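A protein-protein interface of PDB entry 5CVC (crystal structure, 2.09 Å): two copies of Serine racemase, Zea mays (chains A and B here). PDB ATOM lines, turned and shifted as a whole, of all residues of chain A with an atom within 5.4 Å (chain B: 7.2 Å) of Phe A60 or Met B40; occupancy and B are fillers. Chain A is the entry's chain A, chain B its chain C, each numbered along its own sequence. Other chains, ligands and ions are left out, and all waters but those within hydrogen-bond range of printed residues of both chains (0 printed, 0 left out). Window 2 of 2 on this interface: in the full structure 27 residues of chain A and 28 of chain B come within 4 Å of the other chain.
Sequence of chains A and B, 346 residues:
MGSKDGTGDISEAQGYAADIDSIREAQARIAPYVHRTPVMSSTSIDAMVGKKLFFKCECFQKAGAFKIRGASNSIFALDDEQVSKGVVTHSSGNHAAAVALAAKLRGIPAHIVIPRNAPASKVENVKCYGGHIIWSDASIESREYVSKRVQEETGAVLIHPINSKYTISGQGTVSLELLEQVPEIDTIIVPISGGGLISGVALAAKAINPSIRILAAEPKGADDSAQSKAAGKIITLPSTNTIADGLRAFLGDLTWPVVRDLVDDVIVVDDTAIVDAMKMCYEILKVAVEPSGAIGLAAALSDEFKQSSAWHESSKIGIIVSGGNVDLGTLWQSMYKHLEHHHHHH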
ATOM      1  N   HIS A  35      10.883  19.057 -15.882  1.00  0.00           N
ATOM      2  CA  HIS A  35      11.019  19.418 -17.296  1.00  0.00           C
ATOM      3  C   HIS A  35      12.126  18.619 -17.961  1.00  0.00           C
ATOM      4  O   HIS A  35      13.199  18.428 -17.381  1.00  0.00           O
ATOM      5  CB  HIS A  35      11.344  20.902 -17.468  1.00  0.00           C
ATOM      6  CG  HIS A  35      10.248  21.812 -17.019  1.00  0.00           C
ATOM      7  ND1 HIS A  35      10.486  23.027 -16.417  1.00  0.00           N
ATOM      8  CD2 HIS A  35       8.905  21.687 -17.090  1.00  0.00           C
ATOM      9  CE1 HIS A  35       9.336  23.606 -16.123  1.00  0.00           C
ATOM     10  NE2 HIS A  35       8.362  22.817 -16.529  1.00  0.00           N
ATOM     11  N   THR A  37      14.814  19.264 -20.075  1.00  0.00           N
ATOM     12  CA  THR A  37      15.427  20.556 -20.344  1.00  0.00           C
ATOM     13  C   THR A  37      16.148  20.578 -21.688  1.00  0.00           C
ATOM     14  O   THR A  37      16.643  19.543 -22.145  1.00  0.00           O
ATOM     15  CB  THR A  37      16.415  20.945 -19.251  1.00  0.00           C
ATOM     16  OG1 THR A  37      17.401  19.921 -19.131  1.00  0.00           O
ATOM     17  CG2 THR A  37      15.708  21.152 -17.928  1.00  0.00           C
ATOM     18  N   PRO A  38      16.230  21.762 -22.312  1.00  0.00           N
ATOM     19  CA  PRO A  38      16.850  21.886 -23.636  1.00  0.00           C
ATOM     20  C   PRO A  38      18.389  21.875 -23.632  1.00  0.00           C
ATOM     21  O   PRO A  38      19.040  22.075 -22.601  1.00  0.00           O
ATOM     22  CB  PRO A  38      16.344  23.243 -24.132  1.00  0.00           C
ATOM     23  CG  PRO A  38      16.145  24.032 -22.878  1.00  0.00           C
ATOM     24  CD  PRO A  38      15.643  23.036 -21.862  1.00  0.00           C
ATOM     25  N   MET A  40      21.524  23.771 -25.512  1.00  0.00           N
ATOM     26  CA  MET A  40      21.839  24.943 -26.304  1.00  0.00           C
ATOM     27  C   MET A  40      23.303  24.863 -26.716  1.00  0.00           C
ATOM     28  O   MET A  40      24.100  24.148 -26.098  1.00  0.00           O
ATOM     29  CB  MET A  40      21.587  26.224 -25.514  1.00  0.00           C
ATOM     30  CG  MET A  40      20.110  26.503 -25.258  1.00  0.00           C
ATOM     31  SD  MET A  40      19.863  27.940 -24.190  1.00  0.00           S
ATOM     32  CE  MET A  40      20.730  29.207 -25.134  1.00  0.00           C
ATOM     33  N   CYS A  57      20.713  22.605 -20.101  1.00  0.00           N
ATOM     34  CA  CYS A  57      20.246  23.763 -19.332  1.00  0.00           C
ATOM     35  C   CYS A  57      19.335  23.433 -18.167  1.00  0.00           C
ATOM     36  O   CYS A  57      18.134  23.695 -18.223  1.00  0.00           O
ATOM     37  CB  CYS A  57      19.558  24.764 -20.261  1.00  0.00           C
ATOM     38  SG  CYS A  57      20.745  25.502 -21.400  1.00  0.00           S
ATOM     39  N   GLU A  58      19.928  22.923 -17.087  1.00  0.00           N
ATOM     40  CA  GLU A  58      19.170  22.692 -15.842  1.00  0.00           C
ATOM     41  C   GLU A  58      18.772  23.987 -15.103  1.00  0.00           C
ATOM     42  O   GLU A  58      17.928  23.953 -14.187  1.00  0.00           O
ATOM     43  CB  GLU A  58      19.911  21.742 -14.902  1.00  0.00           C
ATOM     44  CG  GLU A  58      20.004  20.320 -15.439  1.00  0.00           C
ATOM     45  CD  GLU A  58      18.651  19.670 -15.633  1.00  0.00           C
ATOM     46  OE1 GLU A  58      17.843  19.516 -14.655  1.00  0.00           O
ATOM     47  OE2 GLU A  58      18.400  19.276 -16.780  1.00  0.00           O
ATOM     48  N   CYS A  59      19.332  25.123 -15.508  1.00  0.00           N
ATOM     49  CA  CYS A  59      18.799  26.407 -15.056  1.00  0.00           C
ATOM     50  C   CYS A  59      17.310  26.563 -15.430  1.00  0.00           C
ATOM     51  O   CYS A  59      16.585  27.283 -14.757  1.00  0.00           O
ATOM     52  CB  CYS A  59      19.612  27.562 -15.639  1.00  0.00           C
ATOM     53  SG  CYS A  59      19.895  27.395 -17.412  1.00  0.00           S
ATOM     54  N   PHE A  60      16.859  25.891 -16.501  1.00  0.00           N
ATOM     55  CA  PHE A  60      15.452  25.961 -16.947  1.00  0.00           C
ATOM     56  C   PHE A  60      14.576  24.870 -16.318  1.00  0.00           C
ATOM     57  O   PHE A  60      13.400  24.734 -16.650  1.00  0.00           O
ATOM     58  CB  PHE A  60      15.353  25.847 -18.483  1.00  0.00           C
ATOM     59  CG  PHE A  60      16.065  26.935 -19.244  1.00  0.00           C
ATOM     60  CD1 PHE A  60      16.173  28.225 -18.743  1.00  0.00           C
ATOM     61  CD2 PHE A  60      16.604  26.668 -20.488  1.00  0.00           C
ATOM     62  CE1 PHE A  60      16.835  29.203 -19.457  1.00  0.00           C
ATOM     63  CE2 PHE A  60      17.248  27.648 -21.217  1.00  0.00           C
ATOM     64  CZ  PHE A  60      17.367  28.920 -20.699  1.00  0.00           C
ATOM     65  N   GLN A  61      15.152  24.094 -15.411  1.00  0.00           N
ATOM     66  CA  GLN A  61      14.420  23.052 -14.712  1.00  0.00           C
ATOM     67  C   GLN A  61      13.549  23.720 -13.669  1.00  0.00           C
ATOM     68  O   GLN A  61      13.798  24.873 -13.306  1.00  0.00           O
ATOM     69  CB  GLN A  61      15.404  22.070 -14.063  1.00  0.00           C
ATOM     70  CG  GLN A  61      14.756  20.922 -13.313  1.00  0.00           C
ATOM     71  CD  GLN A  61      13.846  20.106 -14.212  1.00  0.00           C
ATOM     72  OE1 GLN A  61      12.627  20.279 -14.198  1.00  0.00           O
ATOM     73  NE2 GLN A  61      14.435  19.237 -15.007  1.00  0.00           N
ATOM     74  N   LYS A  62      12.518  23.023 -13.200  1.00  0.00           N
ATOM     75  CA  LYS A  62      11.689  23.552 -12.116  1.00  0.00           C
ATOM     76  C   LYS A  62      12.536  23.927 -10.893  1.00  0.00           C
ATOM     77  O   LYS A  62      13.532  23.264 -10.569  1.00  0.00           O
ATOM     78  CB  LYS A  62      10.604  22.551 -11.714  1.00  0.00           C
ATOM     79  CG  LYS A  62       9.563  22.310 -12.798  1.00  0.00           C
ATOM     80  CD  LYS A  62       8.471  21.380 -12.305  1.00  0.00           C
ATOM     81  CE  LYS A  62       7.492  21.051 -13.410  1.00  0.00           C
ATOM     82  NZ  LYS A  62       6.324  20.313 -12.861  1.00  0.00           N
ATOM     83  N   VAL A 287      21.620  33.152 -21.136  1.00  0.00           N
ATOM     84  CA  VAL A 287      21.066  32.341 -20.048  1.00  0.00           C
ATOM     85  C   VAL A 287      21.460  32.950 -18.699  1.00  0.00           C
ATOM     86  O   VAL A 287      22.643  33.199 -18.429  1.00  0.00           O
ATOM     87  CB  VAL A 287      21.525  30.873 -20.205  1.00  0.00           C
ATOM     88  CG1 VAL A 287      21.009  29.998 -19.076  1.00  0.00           C
ATOM     89  CG2 VAL A 287      21.025  30.324 -21.538  1.00  0.00           C
ATOM     90  N   THR B  37      13.680  29.056 -32.925  1.00  0.00           N
ATOM     91  CA  THR B  37      13.884  29.372 -31.537  1.00  0.00           C
ATOM     92  C   THR B  37      12.828  28.758 -30.640  1.00  0.00           C
ATOM     93  O   THR B  37      11.683  28.551 -31.069  1.00  0.00           O
ATOM     94  CB  THR B  37      13.834  30.879 -31.308  1.00  0.00           C
ATOM     95  OG1 THR B  37      12.575  31.375 -31.781  1.00  0.00           O
ATOM     96  CG2 THR B  37      14.982  31.545 -32.034  1.00  0.00           C
ATOM     97  N   PRO B  38      13.203  28.493 -29.384  1.00  0.00           N
ATOM     98  CA  PRO B  38      12.290  27.771 -28.489  1.00  0.00           C
ATOM     99  C   PRO B  38      11.165  28.645 -27.957  1.00  0.00           C
ATOM    100  O   PRO B  38      11.247  29.890 -27.954  1.00  0.00           O
ATOM    101  CB  PRO B  38      13.190  27.327 -27.334  1.00  0.00           C
ATOM    102  CG  PRO B  38      14.373  28.255 -27.358  1.00  0.00           C
ATOM    103  CD  PRO B  38      14.532  28.731 -28.777  1.00  0.00           C
ATOM    104  N   VAL B  39      10.115  27.973 -27.517  1.00  0.00           N
ATOM    105  CA  VAL B  39       9.026  28.592 -26.795  1.00  0.00           C
ATOM    106  C   VAL B  39       9.170  28.127 -25.357  1.00  0.00           C
ATOM    107  O   VAL B  39       9.345  26.934 -25.122  1.00  0.00           O
ATOM    108  CB  VAL B  39       7.676  28.151 -27.367  1.00  0.00           C
ATOM    109  CG1 VAL B  39       6.532  28.510 -26.428  1.00  0.00           C
ATOM    110  CG2 VAL B  39       7.469  28.780 -28.736  1.00  0.00           C
ATOM    111  N   MET B  40       9.117  29.059 -24.412  1.00  0.00           N
ATOM    112  CA  MET B  40       9.233  28.740 -22.992  1.00  0.00           C
ATOM    113  C   MET B  40       7.969  29.180 -22.265  1.00  0.00           C
ATOM    114  O   MET B  40       7.234  30.030 -22.753  1.00  0.00           O
ATOM    115  CB  MET B  40      10.454  29.431 -22.388  1.00  0.00           C
ATOM    116  CG  MET B  40      11.792  28.951 -22.959  1.00  0.00           C
ATOM    117  SD  MET B  40      13.237  29.699 -22.174  1.00  0.00           S
ATOM    118  CE  MET B  40      12.984  29.267 -20.445  1.00  0.00           C
ATOM    119  N   SER B  41       7.711  28.602 -21.099  1.00  0.00           N
ATOM    120  CA  SER B  41       6.570  29.019 -20.291  1.00  0.00           C
ATOM    121  C   SER B  41       6.876  28.900 -18.808  1.00  0.00           C
ATOM    122  O   SER B  41       7.878  28.290 -18.405  1.00  0.00           O
ATOM    123  CB  SER B  41       5.328  28.207 -20.658  1.00  0.00           C
ATOM    124  OG  SER B  41       5.532  26.826 -20.402  1.00  0.00           O
ATOM    125  N   SER B  42       6.001  29.487 -18.002  1.00  0.00           N
ATOM    126  CA  SER B  42       6.151  29.520 -16.557  1.00  0.00           C
ATOM    127  C   SER B  42       4.767  29.535 -15.898  1.00  0.00           C
ATOM    128  O   SER B  42       3.985  30.469 -16.107  1.00  0.00           O
ATOM    129  CB  SER B  42       6.932  30.763 -16.154  1.00  0.00           C
ATOM    130  OG  SER B  42       6.599  31.204 -14.847  1.00  0.00           O
ATOM    131  N   LEU B  53       0.764  31.817 -20.906  1.00  0.00           N
ATOM    132  CA  LEU B  53       1.722  32.582 -21.689  1.00  0.00           C
ATOM    133  C   LEU B  53       2.744  31.652 -22.342  1.00  0.00           C
ATOM    134  O   LEU B  53       3.180  30.677 -21.739  1.00  0.00           O
ATOM    135  CB  LEU B  53       2.426  33.635 -20.826  1.00  0.00           C
ATOM    136  CG  LEU B  53       1.601  34.703 -20.076  1.00  0.00           C
ATOM    137  CD1 LEU B  53       2.446  35.949 -19.858  1.00  0.00           C
ATOM    138  CD2 LEU B  53       0.316  35.115 -20.770  1.00  0.00           C
ATOM    139  N   PHE B  54       3.112  31.979 -23.578  1.00  0.00           N
ATOM    140  CA  PHE B  54       4.083  31.240 -24.362  1.00  0.00           C
ATOM    141  C   PHE B  54       5.124  32.222 -24.909  1.00  0.00           C
ATOM    142  O   PHE B  54       4.801  33.064 -25.741  1.00  0.00           O
ATOM    143  CB  PHE B  54       3.358  30.508 -25.490  1.00  0.00           C
ATOM    144  CG  PHE B  54       2.409  29.484 -24.980  1.00  0.00           C
ATOM    145  CD1 PHE B  54       2.858  28.207 -24.683  1.00  0.00           C
ATOM    146  CD2 PHE B  54       1.089  29.819 -24.693  1.00  0.00           C
ATOM    147  CE1 PHE B  54       1.999  27.258 -24.150  1.00  0.00           C
ATOM    148  CE2 PHE B  54       0.227  28.873 -24.158  1.00  0.00           C
ATOM    149  CZ  PHE B  54       0.678  27.592 -23.897  1.00  0.00           C
ATOM    150  N   PHE B  55       6.356  32.134 -24.410  1.00  0.00           N
ATOM    151  CA  PHE B  55       7.397  33.098 -24.735  1.00  0.00           C
ATOM    152  C   PHE B  55       8.235  32.618 -25.917  1.00  0.00           C
ATOM    153  O   PHE B  55       8.982  31.660 -25.806  1.00  0.00           O
ATOM    154  CB  PHE B  55       8.310  33.321 -23.523  1.00  0.00           C
ATOM    155  CG  PHE B  55       7.624  33.933 -22.348  1.00  0.00           C
ATOM    156  CD1 PHE B  55       6.969  33.141 -21.414  1.00  0.00           C
ATOM    157  CD2 PHE B  55       7.633  35.310 -22.166  1.00  0.00           C
ATOM    158  CE1 PHE B  55       6.334  33.713 -20.317  1.00  0.00           C
ATOM    159  CE2 PHE B  55       6.998  35.885 -21.079  1.00  0.00           C
ATOM    160  CZ  PHE B  55       6.355  35.088 -20.148  1.00  0.00           C
ATOM    161  N   LYS B  56       8.105  33.290 -27.049  1.00  0.00           N
ATOM    162  CA  LYS B  56       8.881  32.950 -28.245  1.00  0.00           C
ATOM    163  C   LYS B  56      10.230  33.660 -28.115  1.00  0.00           C
ATOM    164  O   LYS B  56      10.297  34.893 -28.137  1.00  0.00           O
ATOM    165  CB  LYS B  56       8.112  33.356 -29.510  1.00  0.00           C
ATOM    166  CG  LYS B  56       8.826  33.128 -30.836  1.00  0.00           C
ATOM    167  CD  LYS B  56       9.183  31.671 -31.073  1.00  0.00           C
ATOM    168  CE  LYS B  56       9.418  31.395 -32.549  1.00  0.00           C
ATOM    169  NZ  LYS B  56      10.179  30.148 -32.753  1.00  0.00           N
ATOM    170  N   CYS B  57      11.290  32.877 -27.926  1.00  0.00           N
ATOM    171  CA  CYS B  57      12.566  33.405 -27.424  1.00  0.00           C
ATOM    172  C   CYS B  57      13.537  33.765 -28.526  1.00  0.00           C
ATOM    173  O   CYS B  57      14.501  33.027 -28.804  1.00  0.00           O
ATOM    174  CB  CYS B  57      13.210  32.409 -26.450  1.00  0.00           C
ATOM    175  SG  CYS B  57      12.273  32.277 -24.908  1.00  0.00           S
ATOM    176  N   CYS B  59      15.556  36.084 -28.272  1.00  0.00           N
ATOM    177  CA  CYS B  59      16.829  36.348 -27.587  1.00  0.00           C
ATOM    178  C   CYS B  59      17.837  35.222 -27.856  1.00  0.00           C
ATOM    179  O   CYS B  59      19.038  35.456 -27.833  1.00  0.00           O
ATOM    180  CB  CYS B  59      16.611  36.535 -26.084  1.00  0.00           C
ATOM    181  SG  CYS B  59      15.609  35.240 -25.349  1.00  0.00           S
ATOM    182  N   PHE B  60      17.334  34.011 -28.113  1.00  0.00           N
ATOM    183  CA  PHE B  60      18.171  32.865 -28.492  1.00  0.00           C
ATOM    184  C   PHE B  60      18.403  32.728 -30.007  1.00  0.00           C
ATOM    185  O   PHE B  60      19.014  31.759 -30.465  1.00  0.00           O
ATOM    186  CB  PHE B  60      17.560  31.565 -27.941  1.00  0.00           C
ATOM    187  CG  PHE B  60      17.399  31.552 -26.434  1.00  0.00           C
ATOM    188  CD1 PHE B  60      18.388  32.063 -25.604  1.00  0.00           C
ATOM    189  CD2 PHE B  60      16.277  31.002 -25.851  1.00  0.00           C
ATOM    190  CE1 PHE B  60      18.245  32.041 -24.229  1.00  0.00           C
ATOM    191  CE2 PHE B  60      16.136  30.972 -24.469  1.00  0.00           C
ATOM    192  CZ  PHE B  60      17.125  31.497 -23.661  1.00  0.00           C
ATOM    193  N   CYS B 281      11.946  37.992 -16.187  1.00  0.00           N
ATOM    194  CA  CYS B 281      12.567  37.145 -17.229  1.00  0.00           C
ATOM    195  C   CYS B 281      13.855  36.517 -16.720  1.00  0.00           C
ATOM    196  O   CYS B 281      14.097  35.343 -16.946  1.00  0.00           O
ATOM    197  CB  CYS B 281      12.885  37.947 -18.492  1.00  0.00           C
ATOM    198  SG  CYS B 281      11.440  38.390 -19.475  1.00  0.00           S
ATOM    199  N   ILE B 284      12.709  34.341 -13.077  1.00  0.00           N
ATOM    200  CA  ILE B 284      11.726  33.278 -13.201  1.00  0.00           C
ATOM    201  C   ILE B 284      12.022  32.405 -14.428  1.00  0.00           C
ATOM    202  O   ILE B 284      12.121  31.189 -14.303  1.00  0.00           O
ATOM    203  CB  ILE B 284      10.284  33.826 -13.285  1.00  0.00           C
ATOM    204  CG1 ILE B 284       9.945  34.714 -12.079  1.00  0.00           C
ATOM    205  CG2 ILE B 284       9.270  32.699 -13.362  1.00  0.00           C
ATOM    206  CD1 ILE B 284      10.131  34.045 -10.730  1.00  0.00           C
ATOM    207  N   LEU B 285      12.167  33.017 -15.604  1.00  0.00           N
ATOM    208  CA  LEU B 285      12.457  32.254 -16.827  1.00  0.00           C
ATOM    209  C   LEU B 285      13.933  31.884 -16.977  1.00  0.00           C
ATOM    210  O   LEU B 285      14.264  30.943 -17.687  1.00  0.00           O
ATOM    211  CB  LEU B 285      12.009  33.039 -18.068  1.00  0.00           C
ATOM    212  CG  LEU B 285      10.528  33.369 -18.157  1.00  0.00           C
ATOM    213  CD1 LEU B 285      10.220  34.232 -19.389  1.00  0.00           C
ATOM    214  CD2 LEU B 285       9.723  32.081 -18.169  1.00  0.00           C
ATOM    215  N   LYS B 286      14.808  32.622 -16.300  1.00  0.00           N
ATOM    216  CA  LYS B 286      16.260  32.429 -16.390  1.00  0.00           C
ATOM    217  C   LYS B 286      16.788  32.826 -17.779  1.00  0.00           C
ATOM    218  O   LYS B 286      17.787  32.292 -18.263  1.00  0.00           O
ATOM    219  CB  LYS B 286      16.669  30.996 -16.020  1.00  0.00           C
ATOM    220  CG  LYS B 286      16.060  30.488 -14.723  1.00  0.00           C
ATOM    221  CD  LYS B 286      16.400  31.391 -13.544  1.00  0.00           C
ATOM    222  CE  LYS B 286      16.055  30.736 -12.218  1.00  0.00           C
ATOM    223  NZ  LYS B 286      16.238  31.677 -11.085  1.00  0.00           N
ATOM    224  N   VAL B 287      16.120  33.796 -18.394  1.00  0.00           N
ATOM    225  CA  VAL B 287      16.484  34.275 -19.731  1.00  0.00           C
ATOM    226  C   VAL B 287      17.027  35.698 -19.622  1.00  0.00           C
ATOM    227  O   VAL B 287      16.330  36.581 -19.122  1.00  0.00           O
ATOM    228  CB  VAL B 287      15.270  34.234 -20.670  1.00  0.00           C
ATOM    229  CG1 VAL B 287      15.648  34.690 -22.071  1.00  0.00           C
ATOM    230  CG2 VAL B 287      14.704  32.823 -20.720  1.00  0.00           C
ATOM    231  N   ALA B 288      18.259  35.903 -20.082  1.00  0.00           N
ATOM    232  CA  ALA B 288      18.945  37.199 -19.991  1.00  0.00           C
ATOM    233  C   ALA B 288      18.572  38.119 -21.161  1.00  0.00           C
ATOM    234  O   ALA B 288      19.355  38.315 -22.110  1.00  0.00           O
ATOM    235  CB  ALA B 288      20.466  37.016 -19.926  1.00  0.00           C
ATOM    236  N   ILE B 319       4.027  35.633 -26.525  1.00  0.00           N
ATOM    237  CA  ILE B 319       4.754  36.848 -26.154  1.00  0.00           C
ATOM    238  C   ILE B 319       6.059  36.796 -26.934  1.00  0.00           C
ATOM    239  O   ILE B 319       6.794  35.832 -26.806  1.00  0.00           O
ATOM    240  CB  ILE B 319       5.107  36.871 -24.657  1.00  0.00           C
ATOM    241  CG1 ILE B 319       3.879  36.631 -23.773  1.00  0.00           C
ATOM    242  CG2 ILE B 319       5.806  38.167 -24.291  1.00  0.00           C
ATOM    243  CD1 ILE B 319       3.033  37.859 -23.493  1.00  0.00           C
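Printed residues of chain A that touch a printed residue of chain B: Met A40, Cys A59, Phe A60 and Val A287.
Hydrophobic or aromatic side chains of chain A that line the printed part of chain B: Met A40 and Phe A60.
Along chain B the printed residues that touch a printed residue of chain A span positions 40 to 286.
Among the printed residues, 7 pairs touch across the chains.
Among the printed residues, no Asp or Glu carboxylate lies within 4 Å of a Lys or Arg side-chain nitrogen of the other chain.
Among the printed residues, pairs that only touch across the chains: Cys A59 with Lys B286 (3.2 Å), Phe A60 with Lys B286 (3.4 Å), Phe A60 with Leu B285 (3.5 Å), Met A40 with Phe B60 (3.7 Å), Val A287 with Lys B286 (3.7 Å), Phe A60 with Met B40 (3.8 Å) and Phe A60 with Phe B60 (3.9 Å).
O of Cys B281 sits at hydrogen-bond distance from N of Lys B286, 2.9 Å away.
A ring nitrogen (ND1) of His A35 is in hydrogen-bond range of the backbone carbonyl oxygen of Phe A60, at 3.4 Å.
O of Met B40 is in hydrogen-bond range of N of Phe B55 (2.8 Å).
Met A40 touches Phe B60, and with the chains exchanged Phe A60 touches Met B40.
Phe B60 touches its own counterpart, Phe A60.
Of the 7 pairs that touch across the chains among the printed residues, 3 have their exchanged pair printed and touching as well.
Phe A60 touches just these residues of chain B: Met B40 (3.8 Å), Phe B60 (3.9 Å), Leu B285 (3.5 Å) and Lys B286 (3.4 Å).
Of chain A, only Phe A60 comes within 4 Å of Met B40.
Printed residues of chain B within 4 Å of Val A287: Lys B286 (3.7 Å).
Printed residues of chain A within 4 Å of Phe B60: Met A40 and Phe A60.
Cys B59 touches none of the printed residues of chain A.
Ile B319 touches none of the printed residues of chain A.
The nearest residue of chain B that does not touch Phe A60 is Val B287 (4.4 Å).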
